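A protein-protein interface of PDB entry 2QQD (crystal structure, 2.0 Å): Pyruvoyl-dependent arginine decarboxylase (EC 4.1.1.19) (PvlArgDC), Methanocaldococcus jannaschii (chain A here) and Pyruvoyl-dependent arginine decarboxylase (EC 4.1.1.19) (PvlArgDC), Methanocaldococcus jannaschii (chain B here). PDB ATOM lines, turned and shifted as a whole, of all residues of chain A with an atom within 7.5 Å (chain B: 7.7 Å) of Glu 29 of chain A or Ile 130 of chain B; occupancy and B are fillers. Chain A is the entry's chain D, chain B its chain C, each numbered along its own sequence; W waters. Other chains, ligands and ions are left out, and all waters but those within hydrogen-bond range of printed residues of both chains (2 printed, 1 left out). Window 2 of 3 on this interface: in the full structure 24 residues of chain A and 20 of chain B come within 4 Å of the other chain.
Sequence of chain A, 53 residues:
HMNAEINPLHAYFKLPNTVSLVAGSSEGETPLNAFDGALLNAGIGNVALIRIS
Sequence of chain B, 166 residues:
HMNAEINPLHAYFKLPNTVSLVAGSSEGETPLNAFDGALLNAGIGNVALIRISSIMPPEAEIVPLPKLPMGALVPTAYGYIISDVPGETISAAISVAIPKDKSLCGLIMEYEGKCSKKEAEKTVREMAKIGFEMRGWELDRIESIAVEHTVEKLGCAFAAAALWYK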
ATOM      1  N   GLU A  27      -3.158 -21.850  23.480  1.00  0.00           N
ATOM      2  CA  GLU A  27      -3.907 -22.646  24.435  1.00  0.00           C
ATOM      3  C   GLU A  27      -5.035 -23.265  23.614  1.00  0.00           C
ATOM      4  O   GLU A  27      -5.265 -22.875  22.466  1.00  0.00           O
ATOM      5  CB  GLU A  27      -4.485 -21.750  25.534  1.00  0.00           C
ATOM      6  CG  GLU A  27      -3.444 -21.185  26.498  1.00  0.00           C
ATOM      7  CD  GLU A  27      -3.102 -22.147  27.630  1.00  0.00           C
ATOM      8  OE1 GLU A  27      -1.898 -22.437  27.828  1.00  0.00           O
ATOM      9  OE2 GLU A  27      -4.037 -22.605  28.327  1.00  0.00           O
ATOM     10  N   GLY A  28      -5.731 -24.232  24.188  1.00  0.00           N
ATOM     11  CA  GLY A  28      -6.830 -24.861  23.481  1.00  0.00           C
ATOM     12  C   GLY A  28      -7.675 -25.637  24.462  1.00  0.00           C
ATOM     13  O   GLY A  28      -7.190 -26.000  25.531  1.00  0.00           O
ATOM     14  N   GLU A  29      -8.928 -25.897  24.106  1.00  0.00           N
ATOM     15  CA  GLU A  29      -9.831 -26.640  24.977  1.00  0.00           C
ATOM     16  C   GLU A  29      -9.583 -28.138  24.860  1.00  0.00           C
ATOM     17  O   GLU A  29     -10.092 -28.933  25.657  1.00  0.00           O
ATOM     18  CB  GLU A  29     -11.280 -26.321  24.622  1.00  0.00           C
ATOM     19  CG  GLU A  29     -11.549 -24.835  24.484  1.00  0.00           C
ATOM     20  CD  GLU A  29     -13.024 -24.503  24.536  1.00  0.00           C
ATOM     21  OE1 GLU A  29     -13.407 -23.412  24.059  1.00  0.00           O
ATOM     22  OE2 GLU A  29     -13.798 -25.331  25.065  1.00  0.00           O
ATOM     23  N   THR A  30      -8.811 -28.516  23.846  1.00  0.00           N
ATOM     24  CA  THR A  30      -8.447 -29.907  23.605  1.00  0.00           C
ATOM     25  C   THR A  30      -7.043 -29.884  23.019  1.00  0.00           C
ATOM     26  O   THR A  30      -6.586 -28.846  22.541  1.00  0.00           O
ATOM     27  CB  THR A  30      -9.386 -30.582  22.584  1.00  0.00           C
ATOM     28  OG1 THR A  30      -9.116 -30.071  21.267  1.00  0.00           O
ATOM     29  CG2 THR A  30     -10.836 -30.327  22.952  1.00  0.00           C
ATOM     30  N   PRO A  31      -6.333 -31.022  23.053  1.00  0.00           N
ATOM     31  CA  PRO A  31      -4.976 -31.048  22.498  1.00  0.00           C
ATOM     32  C   PRO A  31      -4.970 -30.650  21.028  1.00  0.00           C
ATOM     33  O   PRO A  31      -4.162 -29.826  20.608  1.00  0.00           O
ATOM     34  CB  PRO A  31      -4.545 -32.496  22.702  1.00  0.00           C
ATOM     35  CG  PRO A  31      -5.314 -32.905  23.934  1.00  0.00           C
ATOM     36  CD  PRO A  31      -6.677 -32.313  23.669  1.00  0.00           C
ATOM     37  N   LEU A  32      -5.876 -31.234  20.248  1.00  0.00           N
ATOM     38  CA  LEU A  32      -5.944 -30.921  18.823  1.00  0.00           C
ATOM     39  C   LEU A  32      -6.244 -29.444  18.598  1.00  0.00           C
ATOM     40  O   LEU A  32      -5.661 -28.819  17.714  1.00  0.00           O
ATOM     41  CB  LEU A  32      -7.004 -31.786  18.128  1.00  0.00           C
ATOM     42  CG  LEU A  32      -7.060 -31.638  16.599  1.00  0.00           C
ATOM     43  CD1 LEU A  32      -5.694 -31.974  16.009  1.00  0.00           C
ATOM     44  CD2 LEU A  32      -8.124 -32.552  16.015  1.00  0.00           C
ATOM     45  N   ASN A  33      -7.142 -28.873  19.397  1.00  0.00           N
ATOM     46  CA  ASN A  33      -7.464 -27.460  19.238  1.00  0.00           C
ATOM     47  C   ASN A  33      -6.286 -26.576  19.616  1.00  0.00           C
ATOM     48  O   ASN A  33      -6.081 -25.528  19.015  1.00  0.00           O
ATOM     49  CB  ASN A  33      -8.696 -27.077  20.062  1.00  0.00           C
ATOM     50  CG  ASN A  33      -9.990 -27.547  19.422  1.00  0.00           C
ATOM     51  OD1 ASN A  33     -10.288 -27.215  18.262  1.00  0.00           O
ATOM     52  ND2 ASN A  33     -10.764 -28.325  20.164  1.00  0.00           N
ATOM     53  N   ALA A  34      -5.514 -26.992  20.617  1.00  0.00           N
ATOM     54  CA  ALA A  34      -4.347 -26.218  21.026  1.00  0.00           C
ATOM     55  C   ALA A  34      -3.345 -26.247  19.873  1.00  0.00           C
ATOM     56  O   ALA A  34      -2.772 -25.219  19.506  1.00  0.00           O
ATOM     57  CB  ALA A  34      -3.719 -26.830  22.286  1.00  0.00           C
ATOM     58  N   ASP A  36      -3.936 -26.727  16.706  1.00  0.00           N
ATOM     59  CA  ASP A  36      -4.485 -25.896  15.629  1.00  0.00           C
ATOM     60  C   ASP A  36      -4.202 -24.420  15.901  1.00  0.00           C
ATOM     61  O   ASP A  36      -3.812 -23.672  14.996  1.00  0.00           O
ATOM     62  CB  ASP A  36      -6.000 -26.130  15.512  1.00  0.00           C
ATOM     63  CG  ASP A  36      -6.622 -25.405  14.315  1.00  0.00           C
ATOM     64  OD1 ASP A  36      -6.059 -25.491  13.201  1.00  0.00           O
ATOM     65  OD2 ASP A  36      -7.683 -24.763  14.490  1.00  0.00           O
ATOM     66  N   LEU A  40      -1.898 -21.836  13.696  1.00  0.00           N
ATOM     67  CA  LEU A  40      -2.495 -20.552  13.341  1.00  0.00           C
ATOM     68  C   LEU A  40      -1.593 -19.415  13.806  1.00  0.00           C
ATOM     69  O   LEU A  40      -1.286 -18.509  13.033  1.00  0.00           O
ATOM     70  CB  LEU A  40      -3.894 -20.416  13.966  1.00  0.00           C
ATOM     71  CG  LEU A  40      -5.009 -21.221  13.274  1.00  0.00           C
ATOM     72  CD1 LEU A  40      -6.244 -21.272  14.168  1.00  0.00           C
ATOM     73  CD2 LEU A  40      -5.352 -20.589  11.921  1.00  0.00           C
ATOM     74  N   LEU B 107     -12.379 -27.227   7.759  1.00  0.00           N
ATOM     75  CA  LEU B 107     -11.643 -27.777   8.896  1.00  0.00           C
ATOM     76  C   LEU B 107     -12.006 -29.227   9.164  1.00  0.00           C
ATOM     77  O   LEU B 107     -13.166 -29.611   9.085  1.00  0.00           O
ATOM     78  CB  LEU B 107     -11.925 -26.995  10.180  1.00  0.00           C
ATOM     79  CG  LEU B 107     -11.494 -25.536  10.300  1.00  0.00           C
ATOM     80  CD1 LEU B 107     -11.706 -25.091  11.744  1.00  0.00           C
ATOM     81  CD2 LEU B 107     -10.033 -25.387   9.906  1.00  0.00           C
ATOM     82  N   MET B 109     -11.513 -32.348  12.020  1.00  0.00           N
ATOM     83  CA  MET B 109     -11.120 -32.576  13.394  1.00  0.00           C
ATOM     84  C   MET B 109     -11.299 -34.059  13.576  1.00  0.00           C
ATOM     85  O   MET B 109     -12.235 -34.650  13.039  1.00  0.00           O
ATOM     86  CB  MET B 109     -12.023 -31.811  14.369  1.00  0.00           C
ATOM     87  CG  MET B 109     -11.798 -30.298  14.400  1.00  0.00           C
ATOM     88  SD  MET B 109     -10.222 -29.811  15.139  1.00  0.00           S
ATOM     89  CE  MET B 109     -10.246 -28.037  14.854  1.00  0.00           C
ATOM     90  N   THR B 123     -18.168 -34.785  20.768  1.00  0.00           N
ATOM     91  CA  THR B 123     -16.910 -34.097  21.053  1.00  0.00           C
ATOM     92  C   THR B 123     -16.206 -33.573  19.799  1.00  0.00           C
ATOM     93  O   THR B 123     -15.747 -32.432  19.767  1.00  0.00           O
ATOM     94  CB  THR B 123     -15.920 -35.018  21.806  1.00  0.00           C
ATOM     95  OG1 THR B 123     -16.519 -35.482  23.025  1.00  0.00           O
ATOM     96  CG2 THR B 123     -14.643 -34.264  22.134  1.00  0.00           C
ATOM     97  N   VAL B 124     -16.119 -34.400  18.766  1.00  0.00           N
ATOM     98  CA  VAL B 124     -15.435 -33.975  17.547  1.00  0.00           C
ATOM     99  C   VAL B 124     -16.207 -32.844  16.861  1.00  0.00           C
ATOM    100  O   VAL B 124     -15.616 -31.983  16.198  1.00  0.00           O
ATOM    101  CB  VAL B 124     -15.214 -35.182  16.579  1.00  0.00           C
ATOM    102  CG1 VAL B 124     -16.457 -35.439  15.747  1.00  0.00           C
ATOM    103  CG2 VAL B 124     -13.986 -34.925  15.709  1.00  0.00           C
ATOM    104  N   ARG B 125     -17.528 -32.833  17.039  1.00  0.00           N
ATOM    105  CA  ARG B 125     -18.352 -31.774  16.465  1.00  0.00           C
ATOM    106  C   ARG B 125     -18.072 -30.461  17.198  1.00  0.00           C
ATOM    107  O   ARG B 125     -17.997 -29.395  16.576  1.00  0.00           O
ATOM    108  CB  ARG B 125     -19.842 -32.122  16.569  1.00  0.00           C
ATOM    109  CG  ARG B 125     -20.311 -33.194  15.589  1.00  0.00           C
ATOM    110  CD  ARG B 125     -21.830 -33.367  15.628  1.00  0.00           C
ATOM    111  NE  ARG B 125     -22.553 -32.234  15.046  1.00  0.00           N
ATOM    112  CZ  ARG B 125     -22.669 -32.010  13.737  1.00  0.00           C
ATOM    113  NH1 ARG B 125     -22.110 -32.840  12.862  1.00  0.00           N
ATOM    114  NH2 ARG B 125     -23.350 -30.964  13.295  1.00  0.00           N
ATOM    115  N   GLU B 126     -17.902 -30.538  18.513  1.00  0.00           N
ATOM    116  CA  GLU B 126     -17.616 -29.349  19.301  1.00  0.00           C
ATOM    117  C   GLU B 126     -16.238 -28.809  18.931  1.00  0.00           C
ATOM    118  O   GLU B 126     -16.035 -27.604  18.826  1.00  0.00           O
ATOM    119  CB  GLU B 126     -17.662 -29.674  20.795  1.00  0.00           C
ATOM    120  CG  GLU B 126     -17.403 -28.475  21.685  1.00  0.00           C
ATOM    121  CD  GLU B 126     -18.356 -27.330  21.405  1.00  0.00           C
ATOM    122  OE1 GLU B 126     -19.581 -27.563  21.420  1.00  0.00           O
ATOM    123  OE2 GLU B 126     -17.883 -26.199  21.170  1.00  0.00           O
ATOM    124  N   MET B 127     -15.290 -29.717  18.738  1.00  0.00           N
ATOM    125  CA  MET B 127     -13.933 -29.336  18.362  1.00  0.00           C
ATOM    126  C   MET B 127     -13.904 -28.542  17.053  1.00  0.00           C
ATOM    127  O   MET B 127     -13.174 -27.562  16.937  1.00  0.00           O
ATOM    128  CB  MET B 127     -13.060 -30.587  18.241  1.00  0.00           C
ATOM    129  CG  MET B 127     -12.687 -31.183  19.597  1.00  0.00           C
ATOM    130  SD  MET B 127     -12.066 -32.853  19.458  1.00  0.00           S
ATOM    131  CE  MET B 127     -10.410 -32.541  18.804  1.00  0.00           C
ATOM    132  N   ALA B 128     -14.706 -28.956  16.077  1.00  0.00           N
ATOM    133  CA  ALA B 128     -14.749 -28.261  14.793  1.00  0.00           C
ATOM    134  C   ALA B 128     -15.317 -26.857  14.989  1.00  0.00           C
ATOM    135  O   ALA B 128     -14.846 -25.889  14.389  1.00  0.00           O
ATOM    136  CB  ALA B 128     -15.602 -29.041  13.805  1.00  0.00           C
ATOM    137  N   LYS B 129     -16.325 -26.755  15.846  1.00  0.00           N
ATOM    138  CA  LYS B 129     -16.968 -25.485  16.139  1.00  0.00           C
ATOM    139  C   LYS B 129     -15.931 -24.527  16.729  1.00  0.00           C
ATOM    140  O   LYS B 129     -15.835 -23.363  16.325  1.00  0.00           O
ATOM    141  CB  LYS B 129     -18.121 -25.731  17.117  1.00  0.00           C
ATOM    142  CG  LYS B 129     -18.871 -24.503  17.590  1.00  0.00           C
ATOM    143  CD  LYS B 129     -20.019 -24.934  18.502  1.00  0.00           C
ATOM    144  CE  LYS B 129     -20.731 -23.754  19.146  1.00  0.00           C
ATOM    145  NZ  LYS B 129     -21.842 -24.233  20.028  1.00  0.00           N
ATOM    146  N   ILE B 130     -15.151 -25.034  17.680  1.00  0.00           N
ATOM    147  CA  ILE B 130     -14.099 -24.261  18.326  1.00  0.00           C
ATOM    148  C   ILE B 130     -13.057 -23.823  17.297  1.00  0.00           C
ATOM    149  O   ILE B 130     -12.498 -22.733  17.386  1.00  0.00           O
ATOM    150  CB  ILE B 130     -13.402 -25.097  19.430  1.00  0.00           C
ATOM    151  CG1 ILE B 130     -14.380 -25.344  20.583  1.00  0.00           C
ATOM    152  CG2 ILE B 130     -12.150 -24.380  19.918  1.00  0.00           C
ATOM    153  CD1 ILE B 130     -13.942 -26.444  21.537  1.00  0.00           C
ATOM    154  N   GLY B 131     -12.799 -24.684  16.319  1.00  0.00           N
ATOM    155  CA  GLY B 131     -11.834 -24.350  15.287  1.00  0.00           C
ATOM    156  C   GLY B 131     -12.269 -23.117  14.526  1.00  0.00           C
ATOM    157  O   GLY B 131     -11.452 -22.267  14.172  1.00  0.00           O
ATOM    158  N   PHE B 132     -13.568 -23.011  14.270  1.00  0.00           N
ATOM    159  CA  PHE B 132     -14.085 -21.852  13.556  1.00  0.00           C
ATOM    160  C   PHE B 132     -14.119 -20.622  14.464  1.00  0.00           C
ATOM    161  O   PHE B 132     -13.823 -19.508  14.021  1.00  0.00           O
ATOM    162  CB  PHE B 132     -15.476 -22.152  12.991  1.00  0.00           C
ATOM    163  CG  PHE B 132     -15.451 -22.663  11.578  1.00  0.00           C
ATOM    164  CD1 PHE B 132     -14.839 -23.874  11.270  1.00  0.00           C
ATOM    165  CD2 PHE B 132     -16.010 -21.913  10.546  1.00  0.00           C
ATOM    166  CE1 PHE B 132     -14.780 -24.332   9.948  1.00  0.00           C
ATOM    167  CE2 PHE B 132     -15.957 -22.360   9.223  1.00  0.00           C
ATOM    168  CZ  PHE B 132     -15.339 -23.573   8.923  1.00  0.00           C
ATOM    169  N   GLU B 133     -14.465 -20.822  15.733  1.00  0.00           N
ATOM    170  CA  GLU B 133     -14.497 -19.717  16.683  1.00  0.00           C
ATOM    171  C   GLU B 133     -13.108 -19.106  16.816  1.00  0.00           C
ATOM    172  O   GLU B 133     -12.956 -17.884  16.801  1.00  0.00           O
ATOM    173  CB  GLU B 133     -14.983 -20.189  18.056  1.00  0.00           C
ATOM    174  CG  GLU B 133     -16.418 -20.688  18.060  1.00  0.00           C
ATOM    175  CD  GLU B 133     -16.949 -20.957  19.461  1.00  0.00           C
ATOM    176  OE1 GLU B 133     -16.287 -21.696  20.229  1.00  0.00           O
ATOM    177  OE2 GLU B 133     -18.037 -20.431  19.790  1.00  0.00           O
ATOM    178  N   MET B 134     -12.091 -19.957  16.937  1.00  0.00           N
ATOM    179  CA  MET B 134     -10.722 -19.476  17.065  1.00  0.00           C
ATOM    180  C   MET B 134     -10.299 -18.694  15.824  1.00  0.00           C
ATOM    181  O   MET B 134      -9.455 -17.801  15.906  1.00  0.00           O
ATOM    182  CB  MET B 134      -9.760 -20.645  17.314  1.00  0.00           C
ATOM    183  CG  MET B 134      -9.823 -21.202  18.737  1.00  0.00           C
ATOM    184  SD  MET B 134      -8.754 -22.648  19.023  1.00  0.00           S
ATOM    185  CE  MET B 134      -7.150 -21.881  19.104  1.00  0.00           C
ATOM    186  N   ARG B 135     -10.884 -19.022  14.677  1.00  0.00           N
ATOM    187  CA  ARG B 135     -10.544 -18.313  13.441  1.00  0.00           C
ATOM    188  C   ARG B 135     -11.457 -17.103  13.231  1.00  0.00           C
ATOM    189  O   ARG B 135     -11.096 -16.155  12.530  1.00  0.00           O
ATOM    190  CB  ARG B 135     -10.641 -19.262  12.233  1.00  0.00           C
ATOM    191  CG  ARG B 135      -9.506 -20.284  12.141  1.00  0.00           C
ATOM    192  CD  ARG B 135      -9.723 -21.270  10.993  1.00  0.00           C
ATOM    193  NE  ARG B 135      -8.604 -22.195  10.812  1.00  0.00           N
ATOM    194  CZ  ARG B 135      -8.270 -23.157  11.667  1.00  0.00           C
ATOM    195  NH1 ARG B 135      -8.969 -23.333  12.780  1.00  0.00           N
ATOM    196  NH2 ARG B 135      -7.240 -23.953  11.403  1.00  0.00           N
ATOM    197  N   GLY B 136     -12.634 -17.136  13.851  1.00  0.00           N
ATOM    198  CA  GLY B 136     -13.579 -16.045  13.705  1.00  0.00           C
ATOM    199  C   GLY B 136     -14.346 -16.174  12.407  1.00  0.00           C
ATOM    200  O   GLY B 136     -14.844 -15.189  11.862  1.00  0.00           O
ATOM    201  N   LEU B 139     -19.585 -20.351  10.200  1.00  0.00           N
ATOM    202  CA  LEU B 139     -19.766 -21.752   9.874  1.00  0.00           C
ATOM    203  C   LEU B 139     -20.973 -21.947   8.973  1.00  0.00           C
ATOM    204  O   LEU B 139     -21.994 -21.283   9.147  1.00  0.00           O
ATOM    205  CB  LEU B 139     -19.961 -22.549  11.166  1.00  0.00           C
ATOM    206  CG  LEU B 139     -20.031 -24.075  11.107  1.00  0.00           C
ATOM    207  CD1 LEU B 139     -18.705 -24.640  10.624  1.00  0.00           C
ATOM    208  CD2 LEU B 139     -20.360 -24.609  12.510  1.00  0.00           C
ATOM    209  N   ILE B 142     -21.592 -28.586   9.721  1.00  0.00           N
ATOM    210  CA  ILE B 142     -20.615 -29.576  10.126  1.00  0.00           C
ATOM    211  C   ILE B 142     -21.198 -30.964   9.911  1.00  0.00           C
ATOM    212  O   ILE B 142     -22.344 -31.232  10.271  1.00  0.00           O
ATOM    213  CB  ILE B 142     -20.240 -29.429  11.617  1.00  0.00           C
ATOM    214  CG1 ILE B 142     -19.621 -28.050  11.869  1.00  0.00           C
ATOM    215  CG2 ILE B 142     -19.267 -30.538  12.018  1.00  0.00           C
ATOM    216  CD1 ILE B 142     -19.369 -27.746  13.344  1.00  0.00           C
HETATM  217  O   HOH W   1      -9.445 -23.746  21.970  1.00  0.00           O
HETATM  218  O   HOH W   2      -8.328 -27.258  11.655  1.00  0.00           O
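O of Met 127 of chain B sits close to OD1 of Asn 33 of chain A (3.2 Å).
OD2 of Asp 36 of chain A lies within salt-bridge range of NH1 of Arg 135 of chain B, 2.6 Å away.
The side-chain amide nitrogen (ND2) of Asn 33 of chain A lies within hydrogen-bond range of the side-chain hydroxyl (OG1) of Thr 30 of chain A, at 2.6 Å.
O of Gly 131 of chain B is in hydrogen-bond range of NH1 of Arg 135 of chain B.
CE of Met 134 of chain B touches O of Glu 27 of chain A, at 3.98 Å.
CD of Glu 29 of chain A touches CD1 of Ile 130 of chain B, at 3.7 Å.
OG1 of Thr 30 of chain A touches CE of Met 127 of chain B (3.7 Å).
CD2 of Leu 32 of chain A touches SD of Met 109 of chain B, 3.6 Å away.
CB of Leu 32 of chain A touches CE of Met 127 of chain B, at 3.6 Å.
Met 109 of chain B touches Asn 33 of chain A (CE to OD1, 3.5 Å).
Asn 33 of chain A touches Ile 130 of chain B (OD1 to CG2, 3.8 Å).
O of Asn 33 of chain A touches CE of Met 134 of chain B, 3.8 Å away.
CD1 of Leu 40 of chain A touches NH1 of Arg 135 of chain B, at 3.7 Å.
Glu 29 of chain A touches just one residue of chain B: Ile 130.
Of chain A, only Glu 29 and Asn 33 come within 4 Å of Ile 130 of chain B.
No residue of chain B comes within 4 Å of Gly 28 of chain A.
No residue of chain A comes within 4 Å of Gly 131 of chain B.
Of the printed residues of chain B, Glu 27 of chain A touches Met 134.
Printed residues of chain A within 4 Å of Met 109 of chain B: Leu 32 and Asn 33.
Of the printed residues of chain B, Leu 40 of chain A touches Arg 135.
Of the printed residues of chain B, Asp 36 of chain A touches Arg 135.
Leu 139 of chain B touches none of the printed residues of chain A.
Ala 34 of chain A touches none of the printed residues of chain B.
The nearest residue of chain B that does not touch Glu 29 of chain A is Glu 133 of chain B (5.1 Å).
The nearest printed residue of chain A that does not touch Met 109 of chain B is Asp 36 of chain A (4.2 Å).
Of the 18 printed residues of chain B, 5 touch a printed residue of chain A.
Printed residues of chain B that touch a printed residue of chain A: Met 109, Met 127, Ile 130, Met 134 and Arg 135.
Of the 10 printed residues of chain A, 7 touch a printed residue of chain B.
Hydrophobic or aromatic side chains of chain A that line the printed part of chain B: Leu 32 and Leu 40.
Among the printed residues, Asp or Glu carboxylates within 4 Å of a Lys or Arg side-chain nitrogen of the other chain: Asp 36 of chain A with Arg 135 of chain B (2.6 Å).
Water W1 bridges N of Glu 29 of chain A (3.1 Å) and SD of Met 134 of chain B (3.2 Å).
Water W2 lies within hydrogen-bond range of OD1 of Asp 36 of chain A (3.3 Å) and NH2 of Arg 135 of chain B (3.5 Å).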
